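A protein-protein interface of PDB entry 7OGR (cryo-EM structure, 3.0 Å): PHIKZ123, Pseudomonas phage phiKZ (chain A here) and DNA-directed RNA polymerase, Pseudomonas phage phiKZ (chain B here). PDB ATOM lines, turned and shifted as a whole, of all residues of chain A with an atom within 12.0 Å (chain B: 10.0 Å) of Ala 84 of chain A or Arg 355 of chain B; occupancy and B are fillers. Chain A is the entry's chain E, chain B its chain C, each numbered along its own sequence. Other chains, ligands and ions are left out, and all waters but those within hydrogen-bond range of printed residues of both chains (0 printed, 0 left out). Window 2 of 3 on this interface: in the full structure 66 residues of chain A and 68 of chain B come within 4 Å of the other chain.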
ATOM      1  N   PHE A  75      19.229  -4.618   1.296  1.00  0.00           N
ATOM      2  CA  PHE A  75      18.122  -4.701   0.349  1.00  0.00           C
ATOM      3  C   PHE A  75      18.468  -4.035  -0.978  1.00  0.00           C
ATOM      4  O   PHE A  75      18.100  -4.542  -2.045  1.00  0.00           O
ATOM      5  CB  PHE A  75      16.868  -4.070   0.958  1.00  0.00           C
ATOM      6  CG  PHE A  75      15.743  -3.880  -0.022  1.00  0.00           C
ATOM      7  CD1 PHE A  75      15.025  -4.969  -0.491  1.00  0.00           C
ATOM      8  CD2 PHE A  75      15.398  -2.611  -0.465  1.00  0.00           C
ATOM      9  CE1 PHE A  75      13.988  -4.798  -1.392  1.00  0.00           C
ATOM     10  CE2 PHE A  75      14.364  -2.433  -1.365  1.00  0.00           C
ATOM     11  CZ  PHE A  75      13.658  -3.528  -1.829  1.00  0.00           C
ATOM     12  N   GLU A  76      19.175  -2.901  -0.940  1.00  0.00           N
ATOM     13  CA  GLU A  76      19.534  -2.218  -2.177  1.00  0.00           C
ATOM     14  C   GLU A  76      20.661  -2.909  -2.937  1.00  0.00           C
ATOM     15  O   GLU A  76      20.807  -2.674  -4.142  1.00  0.00           O
ATOM     16  CB  GLU A  76      19.922  -0.765  -1.892  1.00  0.00           C
ATOM     17  CG  GLU A  76      18.768   0.099  -1.408  1.00  0.00           C
ATOM     18  CD  GLU A  76      17.808   0.465  -2.523  1.00  0.00           C
ATOM     19  OE1 GLU A  76      18.267   0.648  -3.668  1.00  0.00           O
ATOM     20  OE2 GLU A  76      16.593   0.569  -2.251  1.00  0.00           O
ATOM     21  N   ILE A  78      21.045  -6.473  -2.764  1.00  0.00           N
ATOM     22  CA  ILE A  78      20.454  -7.703  -3.286  1.00  0.00           C
ATOM     23  C   ILE A  78      19.644  -7.407  -4.544  1.00  0.00           C
ATOM     24  O   ILE A  78      19.838  -8.035  -5.591  1.00  0.00           O
ATOM     25  CB  ILE A  78      19.600  -8.400  -2.208  1.00  0.00           C
ATOM     26  CG1 ILE A  78      20.496  -9.110  -1.191  1.00  0.00           C
ATOM     27  CG2 ILE A  78      18.635  -9.403  -2.835  1.00  0.00           C
ATOM     28  CD1 ILE A  78      19.726  -9.893  -0.141  1.00  0.00           C
ATOM     29  N   THR A  79      18.741  -6.429  -4.466  1.00  0.00           N
ATOM     30  CA  THR A  79      17.869  -6.074  -5.585  1.00  0.00           C
ATOM     31  C   THR A  79      18.485  -4.890  -6.325  1.00  0.00           C
ATOM     32  O   THR A  79      18.097  -3.735  -6.151  1.00  0.00           O
ATOM     33  CB  THR A  79      16.463  -5.758  -5.087  1.00  0.00           C
ATOM     34  OG1 THR A  79      16.442  -4.446  -4.512  1.00  0.00           O
ATOM     35  CG2 THR A  79      16.029  -6.771  -4.038  1.00  0.00           C
ATOM     36  N   ARG A  80      19.468  -5.194  -7.167  1.00  0.00           N
ATOM     37  CA  ARG A  80      20.168  -4.194  -7.962  1.00  0.00           C
ATOM     38  C   ARG A  80      19.713  -4.293  -9.412  1.00  0.00           C
ATOM     39  O   ARG A  80      19.681  -5.388  -9.982  1.00  0.00           O
ATOM     40  CB  ARG A  80      21.686  -4.379  -7.858  1.00  0.00           C
ATOM     41  CG  ARG A  80      22.489  -3.683  -8.951  1.00  0.00           C
ATOM     42  CD  ARG A  80      23.855  -3.248  -8.449  1.00  0.00           C
ATOM     43  NE  ARG A  80      23.768  -2.075  -7.583  1.00  0.00           N
ATOM     44  CZ  ARG A  80      24.650  -1.779  -6.635  1.00  0.00           C
ATOM     45  NH1 ARG A  80      24.490  -0.690  -5.894  1.00  0.00           N
ATOM     46  NH2 ARG A  80      25.693  -2.570  -6.428  1.00  0.00           N
ATOM     47  N   GLU A  81      19.350  -3.152  -9.996  1.00  0.00           N
ATOM     48  CA  GLU A  81      18.923  -3.105 -11.389  1.00  0.00           C
ATOM     49  C   GLU A  81      20.113  -3.345 -12.311  1.00  0.00           C
ATOM     50  O   GLU A  81      21.069  -2.562 -12.319  1.00  0.00           O
ATOM     51  CB  GLU A  81      18.272  -1.757 -11.691  1.00  0.00           C
ATOM     52  CG  GLU A  81      17.947  -1.535 -13.158  1.00  0.00           C
ATOM     53  CD  GLU A  81      17.279  -0.199 -13.410  1.00  0.00           C
ATOM     54  OE1 GLU A  81      17.021   0.533 -12.433  1.00  0.00           O
ATOM     55  OE2 GLU A  81      17.013   0.121 -14.587  1.00  0.00           O
ATOM     56  N   TYR A  82      20.058  -4.429 -13.085  1.00  0.00           N
ATOM     57  CA  TYR A  82      21.140  -4.802 -13.987  1.00  0.00           C
ATOM     58  C   TYR A  82      20.786  -4.546 -15.446  1.00  0.00           C
ATOM     59  O   TYR A  82      21.526  -3.852 -16.150  1.00  0.00           O
ATOM     60  CB  TYR A  82      21.504  -6.280 -13.777  1.00  0.00           C
ATOM     61  CG  TYR A  82      22.429  -6.844 -14.833  1.00  0.00           C
ATOM     62  CD1 TYR A  82      23.722  -6.353 -14.988  1.00  0.00           C
ATOM     63  CD2 TYR A  82      22.009  -7.865 -15.678  1.00  0.00           C
ATOM     64  CE1 TYR A  82      24.571  -6.867 -15.955  1.00  0.00           C
ATOM     65  CE2 TYR A  82      22.851  -8.385 -16.647  1.00  0.00           C
ATOM     66  CZ  TYR A  82      24.129  -7.881 -16.780  1.00  0.00           C
ATOM     67  OH  TYR A  82      24.966  -8.397 -17.741  1.00  0.00           O
ATOM     68  N   ASN A  83      19.669  -5.090 -15.920  1.00  0.00           N
ATOM     69  CA  ASN A  83      19.227  -4.961 -17.305  1.00  0.00           C
ATOM     70  C   ASN A  83      17.792  -4.437 -17.322  1.00  0.00           C
ATOM     71  O   ASN A  83      16.896  -5.014 -17.943  1.00  0.00           O
ATOM     72  CB  ASN A  83      19.372  -6.302 -18.031  1.00  0.00           C
ATOM     73  CG  ASN A  83      19.241  -6.186 -19.553  1.00  0.00           C
ATOM     74  OD1 ASN A  83      18.871  -5.144 -20.093  1.00  0.00           O
ATOM     75  ND2 ASN A  83      19.555  -7.271 -20.246  1.00  0.00           N
ATOM     76  N   ALA A  84      17.579  -3.341 -16.574  1.00  0.00           N
ATOM     77  CA  ALA A  84      16.270  -2.709 -16.344  1.00  0.00           C
ATOM     78  C   ALA A  84      15.270  -3.688 -15.731  1.00  0.00           C
ATOM     79  O   ALA A  84      14.078  -3.672 -16.047  1.00  0.00           O
ATOM     80  CB  ALA A  84      15.706  -2.069 -17.620  1.00  0.00           C
ATOM     81  N   LYS A  85      15.764  -4.546 -14.840  1.00  0.00           N
ATOM     82  CA  LYS A  85      14.931  -5.536 -14.166  1.00  0.00           C
ATOM     83  C   LYS A  85      15.584  -5.860 -12.832  1.00  0.00           C
ATOM     84  O   LYS A  85      16.725  -6.328 -12.800  1.00  0.00           O
ATOM     85  CB  LYS A  85      14.775  -6.797 -15.019  1.00  0.00           C
ATOM     86  CG  LYS A  85      13.814  -7.834 -14.458  1.00  0.00           C
ATOM     87  CD  LYS A  85      13.630  -8.984 -15.437  1.00  0.00           C
ATOM     88  CE  LYS A  85      12.754 -10.083 -14.859  1.00  0.00           C
ATOM     89  NZ  LYS A  85      11.351  -9.630 -14.661  1.00  0.00           N
ATOM     90  N   ARG A  86      14.866  -5.614 -11.741  1.00  0.00           N
ATOM     91  CA  ARG A  86      15.398  -5.786 -10.391  1.00  0.00           C
ATOM     92  C   ARG A  86      14.987  -7.165  -9.892  1.00  0.00           C
ATOM     93  O   ARG A  86      13.859  -7.362  -9.433  1.00  0.00           O
ATOM     94  CB  ARG A  86      14.902  -4.680  -9.467  1.00  0.00           C
ATOM     95  CG  ARG A  86      15.355  -3.289  -9.874  1.00  0.00           C
ATOM     96  CD  ARG A  86      14.847  -2.235  -8.909  1.00  0.00           C
ATOM     97  NE  ARG A  86      15.190  -2.547  -7.526  1.00  0.00           N
ATOM     98  CZ  ARG A  86      14.674  -1.926  -6.471  1.00  0.00           C
ATOM     99  NH1 ARG A  86      15.045  -2.276  -5.247  1.00  0.00           N
ATOM    100  NH2 ARG A  86      13.788  -0.956  -6.641  1.00  0.00           N
ATOM    101  N   ILE A  87      15.911  -8.119  -9.983  1.00  0.00           N
ATOM    102  CA  ILE A  87      15.644  -9.503  -9.612  1.00  0.00           C
ATOM    103  C   ILE A  87      15.591  -9.639  -8.097  1.00  0.00           C
ATOM    104  O   ILE A  87      16.627  -9.630  -7.424  1.00  0.00           O
ATOM    105  CB  ILE A  87      16.705 -10.452 -10.201  1.00  0.00           C
ATOM    106  CG1 ILE A  87      16.830 -10.248 -11.711  1.00  0.00           C
ATOM    107  CG2 ILE A  87      16.360 -11.900  -9.886  1.00  0.00           C
ATOM    108  CD1 ILE A  87      15.568 -10.567 -12.466  1.00  0.00           C
ATOM    109  N   ALA A  88      14.385  -9.755  -7.554  1.00  0.00           N
ATOM    110  CA  ALA A  88      14.214 -10.146  -6.166  1.00  0.00           C
ATOM    111  C   ALA A  88      14.105 -11.664  -6.072  1.00  0.00           C
ATOM    112  O   ALA A  88      13.726 -12.344  -7.028  1.00  0.00           O
ATOM    113  CB  ALA A  88      12.974  -9.486  -5.561  1.00  0.00           C
ATOM    114  N   ASP B 286       1.726  -8.457  -6.222  1.00  0.00           N
ATOM    115  CA  ASP B 286       2.429  -7.500  -7.076  1.00  0.00           C
ATOM    116  C   ASP B 286       1.428  -6.416  -7.454  1.00  0.00           C
ATOM    117  O   ASP B 286       0.689  -6.533  -8.432  1.00  0.00           O
ATOM    118  CB  ASP B 286       3.014  -8.192  -8.301  1.00  0.00           C
ATOM    119  CG  ASP B 286       3.668  -7.221  -9.266  1.00  0.00           C
ATOM    120  OD1 ASP B 286       4.292  -6.245  -8.801  1.00  0.00           O
ATOM    121  OD2 ASP B 286       3.554  -7.435 -10.491  1.00  0.00           O
ATOM    122  N   ARG B 288       1.866  -3.361  -8.573  1.00  0.00           N
ATOM    123  CA  ARG B 288       2.396  -2.313  -9.436  1.00  0.00           C
ATOM    124  C   ARG B 288       1.895  -2.432 -10.871  1.00  0.00           C
ATOM    125  O   ARG B 288       2.413  -1.751 -11.761  1.00  0.00           O
ATOM    126  CB  ARG B 288       3.924  -2.309  -9.410  1.00  0.00           C
ATOM    127  CG  ARG B 288       4.510  -1.571  -8.221  1.00  0.00           C
ATOM    128  CD  ARG B 288       4.538  -0.071  -8.477  1.00  0.00           C
ATOM    129  NE  ARG B 288       5.637   0.327  -9.351  1.00  0.00           N
ATOM    130  CZ  ARG B 288       6.822   0.744  -8.918  1.00  0.00           C
ATOM    131  NH1 ARG B 288       7.762   1.087  -9.786  1.00  0.00           N
ATOM    132  NH2 ARG B 288       7.066   0.822  -7.617  1.00  0.00           N
ATOM    133  N   GLN B 345      11.323  -5.112   3.541  1.00  0.00           N
ATOM    134  CA  GLN B 345      11.468  -4.228   2.391  1.00  0.00           C
ATOM    135  C   GLN B 345      11.176  -4.934   1.075  1.00  0.00           C
ATOM    136  O   GLN B 345      10.795  -4.271   0.104  1.00  0.00           O
ATOM    137  CB  GLN B 345      12.872  -3.622   2.338  1.00  0.00           C
ATOM    138  CG  GLN B 345      13.185  -2.645   3.458  1.00  0.00           C
ATOM    139  CD  GLN B 345      14.662  -2.312   3.536  1.00  0.00           C
ATOM    140  OE1 GLN B 345      15.211  -1.672   2.640  1.00  0.00           O
ATOM    141  NE2 GLN B 345      15.313  -2.754   4.600  1.00  0.00           N
ATOM    142  N   LEU B 348       6.972  -4.862   0.974  1.00  0.00           N
ATOM    143  CA  LEU B 348       6.257  -3.611   0.778  1.00  0.00           C
ATOM    144  C   LEU B 348       6.549  -3.022  -0.603  1.00  0.00           C
ATOM    145  O   LEU B 348       7.648  -3.191  -1.137  1.00  0.00           O
ATOM    146  CB  LEU B 348       6.639  -2.608   1.863  1.00  0.00           C
ATOM    147  CG  LEU B 348       6.353  -3.048   3.300  1.00  0.00           C
ATOM    148  CD1 LEU B 348       6.876  -2.018   4.289  1.00  0.00           C
ATOM    149  CD2 LEU B 348       4.867  -3.299   3.505  1.00  0.00           C
ATOM    150  N   PRO B 349       5.573  -2.340  -1.208  1.00  0.00           N
ATOM    151  CA  PRO B 349       5.802  -1.751  -2.532  1.00  0.00           C
ATOM    152  C   PRO B 349       6.718  -0.541  -2.469  1.00  0.00           C
ATOM    153  O   PRO B 349       6.783   0.176  -1.467  1.00  0.00           O
ATOM    154  CB  PRO B 349       4.394  -1.354  -2.993  1.00  0.00           C
ATOM    155  CG  PRO B 349       3.618  -1.193  -1.732  1.00  0.00           C
ATOM    156  CD  PRO B 349       4.164  -2.220  -0.792  1.00  0.00           C
ATOM    157  N   GLN B 350       7.435  -0.328  -3.559  1.00  0.00           N
ATOM    158  CA  GLN B 350       8.378   0.765  -3.727  1.00  0.00           C
ATOM    159  C   GLN B 350       7.661   2.010  -4.227  1.00  0.00           C
ATOM    160  O   GLN B 350       6.570   1.924  -4.800  1.00  0.00           O
ATOM    161  CB  GLN B 350       9.475   0.366  -4.716  1.00  0.00           C
ATOM    162  CG  GLN B 350      10.532  -0.593  -4.180  1.00  0.00           C
ATOM    163  CD  GLN B 350      10.042  -2.023  -4.092  1.00  0.00           C
ATOM    164  OE1 GLN B 350      10.108  -2.652  -3.037  1.00  0.00           O
ATOM    165  NE2 GLN B 350       9.522  -2.535  -5.201  1.00  0.00           N
ATOM    166  N   PRO B 351       8.235   3.192  -4.011  1.00  0.00           N
ATOM    167  CA  PRO B 351       7.744   4.383  -4.711  1.00  0.00           C
ATOM    168  C   PRO B 351       8.026   4.297  -6.206  1.00  0.00           C
ATOM    169  O   PRO B 351       8.862   3.518  -6.669  1.00  0.00           O
ATOM    170  CB  PRO B 351       8.522   5.534  -4.062  1.00  0.00           C
ATOM    171  CG  PRO B 351       9.689   4.883  -3.387  1.00  0.00           C
ATOM    172  CD  PRO B 351       9.198   3.542  -2.952  1.00  0.00           C
ATOM    173  N   ASP B 352       7.317   5.132  -6.965  1.00  0.00           N
ATOM    174  CA  ASP B 352       7.343   5.071  -8.423  1.00  0.00           C
ATOM    175  C   ASP B 352       8.577   5.750  -9.027  1.00  0.00           C
ATOM    176  O   ASP B 352       8.663   5.877 -10.252  1.00  0.00           O
ATOM    177  CB  ASP B 352       6.066   5.703  -8.988  1.00  0.00           C
ATOM    178  CG  ASP B 352       5.554   4.996 -10.237  1.00  0.00           C
ATOM    179  OD1 ASP B 352       4.327   5.029 -10.467  1.00  0.00           O
ATOM    180  OD2 ASP B 352       6.353   4.382 -10.973  1.00  0.00           O
ATOM    181  N   ASN B 353       9.526   6.196  -8.204  1.00  0.00           N
ATOM    182  CA  ASN B 353      10.761   6.772  -8.719  1.00  0.00           C
ATOM    183  C   ASN B 353      11.740   5.714  -9.209  1.00  0.00           C
ATOM    184  O   ASN B 353      12.613   6.027 -10.025  1.00  0.00           O
ATOM    185  CB  ASN B 353      11.432   7.628  -7.642  1.00  0.00           C
ATOM    186  CG  ASN B 353      10.649   8.886  -7.325  1.00  0.00           C
ATOM    187  OD1 ASN B 353      10.131   9.551  -8.223  1.00  0.00           O
ATOM    188  ND2 ASN B 353      10.557   9.219  -6.043  1.00  0.00           N
ATOM    189  N   VAL B 354      11.614   4.476  -8.729  1.00  0.00           N
ATOM    190  CA  VAL B 354      12.520   3.396  -9.106  1.00  0.00           C
ATOM    191  C   VAL B 354      11.731   2.285  -9.785  1.00  0.00           C
ATOM    192  O   VAL B 354      10.499   2.354  -9.884  1.00  0.00           O
ATOM    193  CB  VAL B 354      13.285   2.853  -7.883  1.00  0.00           C
ATOM    194  CG1 VAL B 354      14.047   3.968  -7.184  1.00  0.00           C
ATOM    195  CG2 VAL B 354      12.331   2.174  -6.914  1.00  0.00           C
ATOM    196  N   ARG B 355      12.433   1.262 -10.264  1.00  0.00           N
ATOM    197  CA  ARG B 355      11.778   0.110 -10.863  1.00  0.00           C
ATOM    198  C   ARG B 355      11.119  -0.752  -9.788  1.00  0.00           C
ATOM    199  O   ARG B 355      11.494  -0.726  -8.612  1.00  0.00           O
ATOM    200  CB  ARG B 355      12.781  -0.728 -11.657  1.00  0.00           C
ATOM    201  CG  ARG B 355      13.272  -0.082 -12.943  1.00  0.00           C
ATOM    202  CD  ARG B 355      12.146   0.080 -13.949  1.00  0.00           C
ATOM    203  NE  ARG B 355      12.612   0.678 -15.195  1.00  0.00           N
ATOM    204  CZ  ARG B 355      12.773   0.008 -16.331  1.00  0.00           C
ATOM    205  NH1 ARG B 355      13.204   0.634 -17.417  1.00  0.00           N
ATOM    206  NH2 ARG B 355      12.503  -1.289 -16.381  1.00  0.00           N
ATOM    207  N   LYS B 356      10.120  -1.522 -10.209  1.00  0.00           N
ATOM    208  CA  LYS B 356       9.435  -2.423  -9.297  1.00  0.00           C
ATOM    209  C   LYS B 356      10.188  -3.745  -9.187  1.00  0.00           C
ATOM    210  O   LYS B 356      11.000  -4.105 -10.043  1.00  0.00           O
ATOM    211  CB  LYS B 356       7.999  -2.674  -9.762  1.00  0.00           C
ATOM    212  CG  LYS B 356       7.883  -3.239 -11.167  1.00  0.00           C
ATOM    213  CD  LYS B 356       6.689  -4.175 -11.280  1.00  0.00           C
ATOM    214  CE  LYS B 356       6.521  -4.703 -12.696  1.00  0.00           C
ATOM    215  NZ  LYS B 356       7.698  -5.498 -13.145  1.00  0.00           N
ATOM    216  N   LEU B 357       9.905  -4.473  -8.111  1.00  0.00           N
ATOM    217  CA  LEU B 357      10.583  -5.734  -7.849  1.00  0.00           C
ATOM    218  C   LEU B 357      10.010  -6.854  -8.707  1.00  0.00           C
ATOM    219  O   LEU B 357       8.792  -6.990  -8.848  1.00  0.00           O
ATOM    220  CB  LEU B 357      10.470  -6.108  -6.371  1.00  0.00           C
ATOM    221  CG  LEU B 357      11.379  -5.369  -5.388  1.00  0.00           C
ATOM    222  CD1 LEU B 357      11.296  -5.994  -4.005  1.00  0.00           C
ATOM    223  CD2 LEU B 357      12.812  -5.350  -5.888  1.00  0.00           C
ATOM    224  N   SER B 358      10.903  -7.658  -9.279  1.00  0.00           N
ATOM    225  CA  SER B 358      10.535  -8.881  -9.988  1.00  0.00           C
ATOM    226  C   SER B 358      10.835 -10.040  -9.044  1.00  0.00           C
ATOM    227  O   SER B 358      11.935 -10.594  -9.038  1.00  0.00           O
ATOM    228  CB  SER B 358      11.293  -9.003 -11.304  1.00  0.00           C
ATOM    229  OG  SER B 358      11.007  -7.913 -12.160  1.00  0.00           O
ATOM    230  N   ARG B 359       9.845 -10.399  -8.233  1.00  0.00           N
ATOM    231  CA  ARG B 359      10.041 -11.383  -7.179  1.00  0.00           C
ATOM    232  C   ARG B 359       9.998 -12.801  -7.736  1.00  0.00           C
ATOM    233  O   ARG B 359       9.221 -13.106  -8.644  1.00  0.00           O
ATOM    234  CB  ARG B 359       8.980 -11.204  -6.095  1.00  0.00           C
ATOM    235  CG  ARG B 359       8.890  -9.778  -5.575  1.00  0.00           C
ATOM    236  CD  ARG B 359       7.700  -9.581  -4.654  1.00  0.00           C
ATOM    237  NE  ARG B 359       7.367  -8.167  -4.504  1.00  0.00           N
ATOM    238  CZ  ARG B 359       6.281  -7.715  -3.885  1.00  0.00           C
ATOM    239  NH1 ARG B 359       6.061  -6.411  -3.797  1.00  0.00           N
ATOM    240  NH2 ARG B 359       5.415  -8.566  -3.353  1.00  0.00           N
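Of chain B, only Arg 355 comes within 4 Å of Ala 84 of chain A. Gln 350 of chain B touches one residue of chain A. Of chain A, only Phe 75 (3.9 Å), Thr 79 (3.8 Å) and Arg 86 (3.9 Å) come within 4 Å of Leu 357 of chain B. Printed residues of chain A within 4 Å of Arg 359 of chain B: Ala 88 (3.8 Å). Of the printed residues of chain A, Lys 356 of chain B touches Arg 86. Printed residues of chain B within 4 Å of Ile 87 of chain A: Ser 358. Printed residues of chain A within 4 Å of Gln 345 of chain B: Phe 75. Of the printed residues of chain B, Phe 75 of chain A touches Gln 345 (3.2 Å), Gln 350 (3.9 Å) and Leu 357 (3.9 Å). Pro 351 of chain B touches none of the printed residues of chain A. Asp 286 of chain B touches none of the printed residues of chain A. The nearest residue of chain B that does not touch Ala 84 of chain A is Ser 358 of chain B (6.5 Å).
OE1 of Gln 345 of chain B touches CD2 of Phe 75 of chain A (3.2 Å). Gln 350 of chain B touches Phe 75 of chain A. Phe 75 of chain A touches Leu 357 of chain B (CE1 to CD1, 3.9 Å). CD2 of Leu 357 of chain B touches CB of Thr 79 of chain A (3.8 Å). Glu 81 of chain A touches Arg 355 of chain B (OE1 to CG, 3.8 Å). Val 354 of chain B touches Arg 86 of chain A (CG2 to NH2, 3.5 Å). O of Lys 356 of chain B touches CB of Arg 86 of chain A, at 3.99 Å. Arg 86 of chain A touches Leu 357 of chain B. Ile 87 of chain A touches Ser 358 of chain B. Ala 88 of chain A touches Arg 359 of chain B.
Hydrophobic or aromatic side chains of chain A within 4 Å of the printed part of chain B: Phe 75, Ala 84 and Ala 88. Hydrophobic or aromatic side chains of chain B within 4 Å of the printed part of chain A: Val 354 and Leu 357. Among the printed residues, 15 pairs touch across the chains.
The side-chain amino group of Lys 85 of chain A lies within hydrogen-bond range of the side-chain hydroxyl of Ser 358 of chain B. The backbone carbonyl oxygen of Arg 355 of chain B is in hydrogen-bond range of the guanidinium group of Arg 86 of chain A (3.0 Å). O of Ala 84 of chain A sits at hydrogen-bond distance from NH2 of Arg 355 of chain B, 2.9 Å away. O of Ser 358 of chain B is in hydrogen-bond range of N of Ala 88 of chain A (3.0 Å). The backbone NH (N) of Ser 358 of chain B lies within hydrogen-bond range of the backbone carbonyl oxygen (O) of Arg 86 of chain A.
OG1 of Thr 79 of chain A is in hydrogen-bond range of NH1 of Arg 86 of chain A (2.7 Å). The guanidinium group (NH2) of Arg 288 of chain B lies within hydrogen-bond range of the backbone carbonyl oxygen (O) of Gln 350 of chain B, 3.1 Å away. The backbone carbonyl oxygen (O) of Phe 75 of chain A sits at hydrogen-bond distance from the side-chain hydroxyl (OG1) of Thr 79 of chain A (3.0 Å). The guanidinium group (NH1) of Arg 288 of chain B sits at hydrogen-bond distance from the backbone carbonyl oxygen (O) of Val 354 of chain B. The backbone carbonyl oxygen (O) of Leu 348 of chain B lies close to the side-chain amide oxygen (OE1) of Gln 350 of chain B (3.2 Å).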
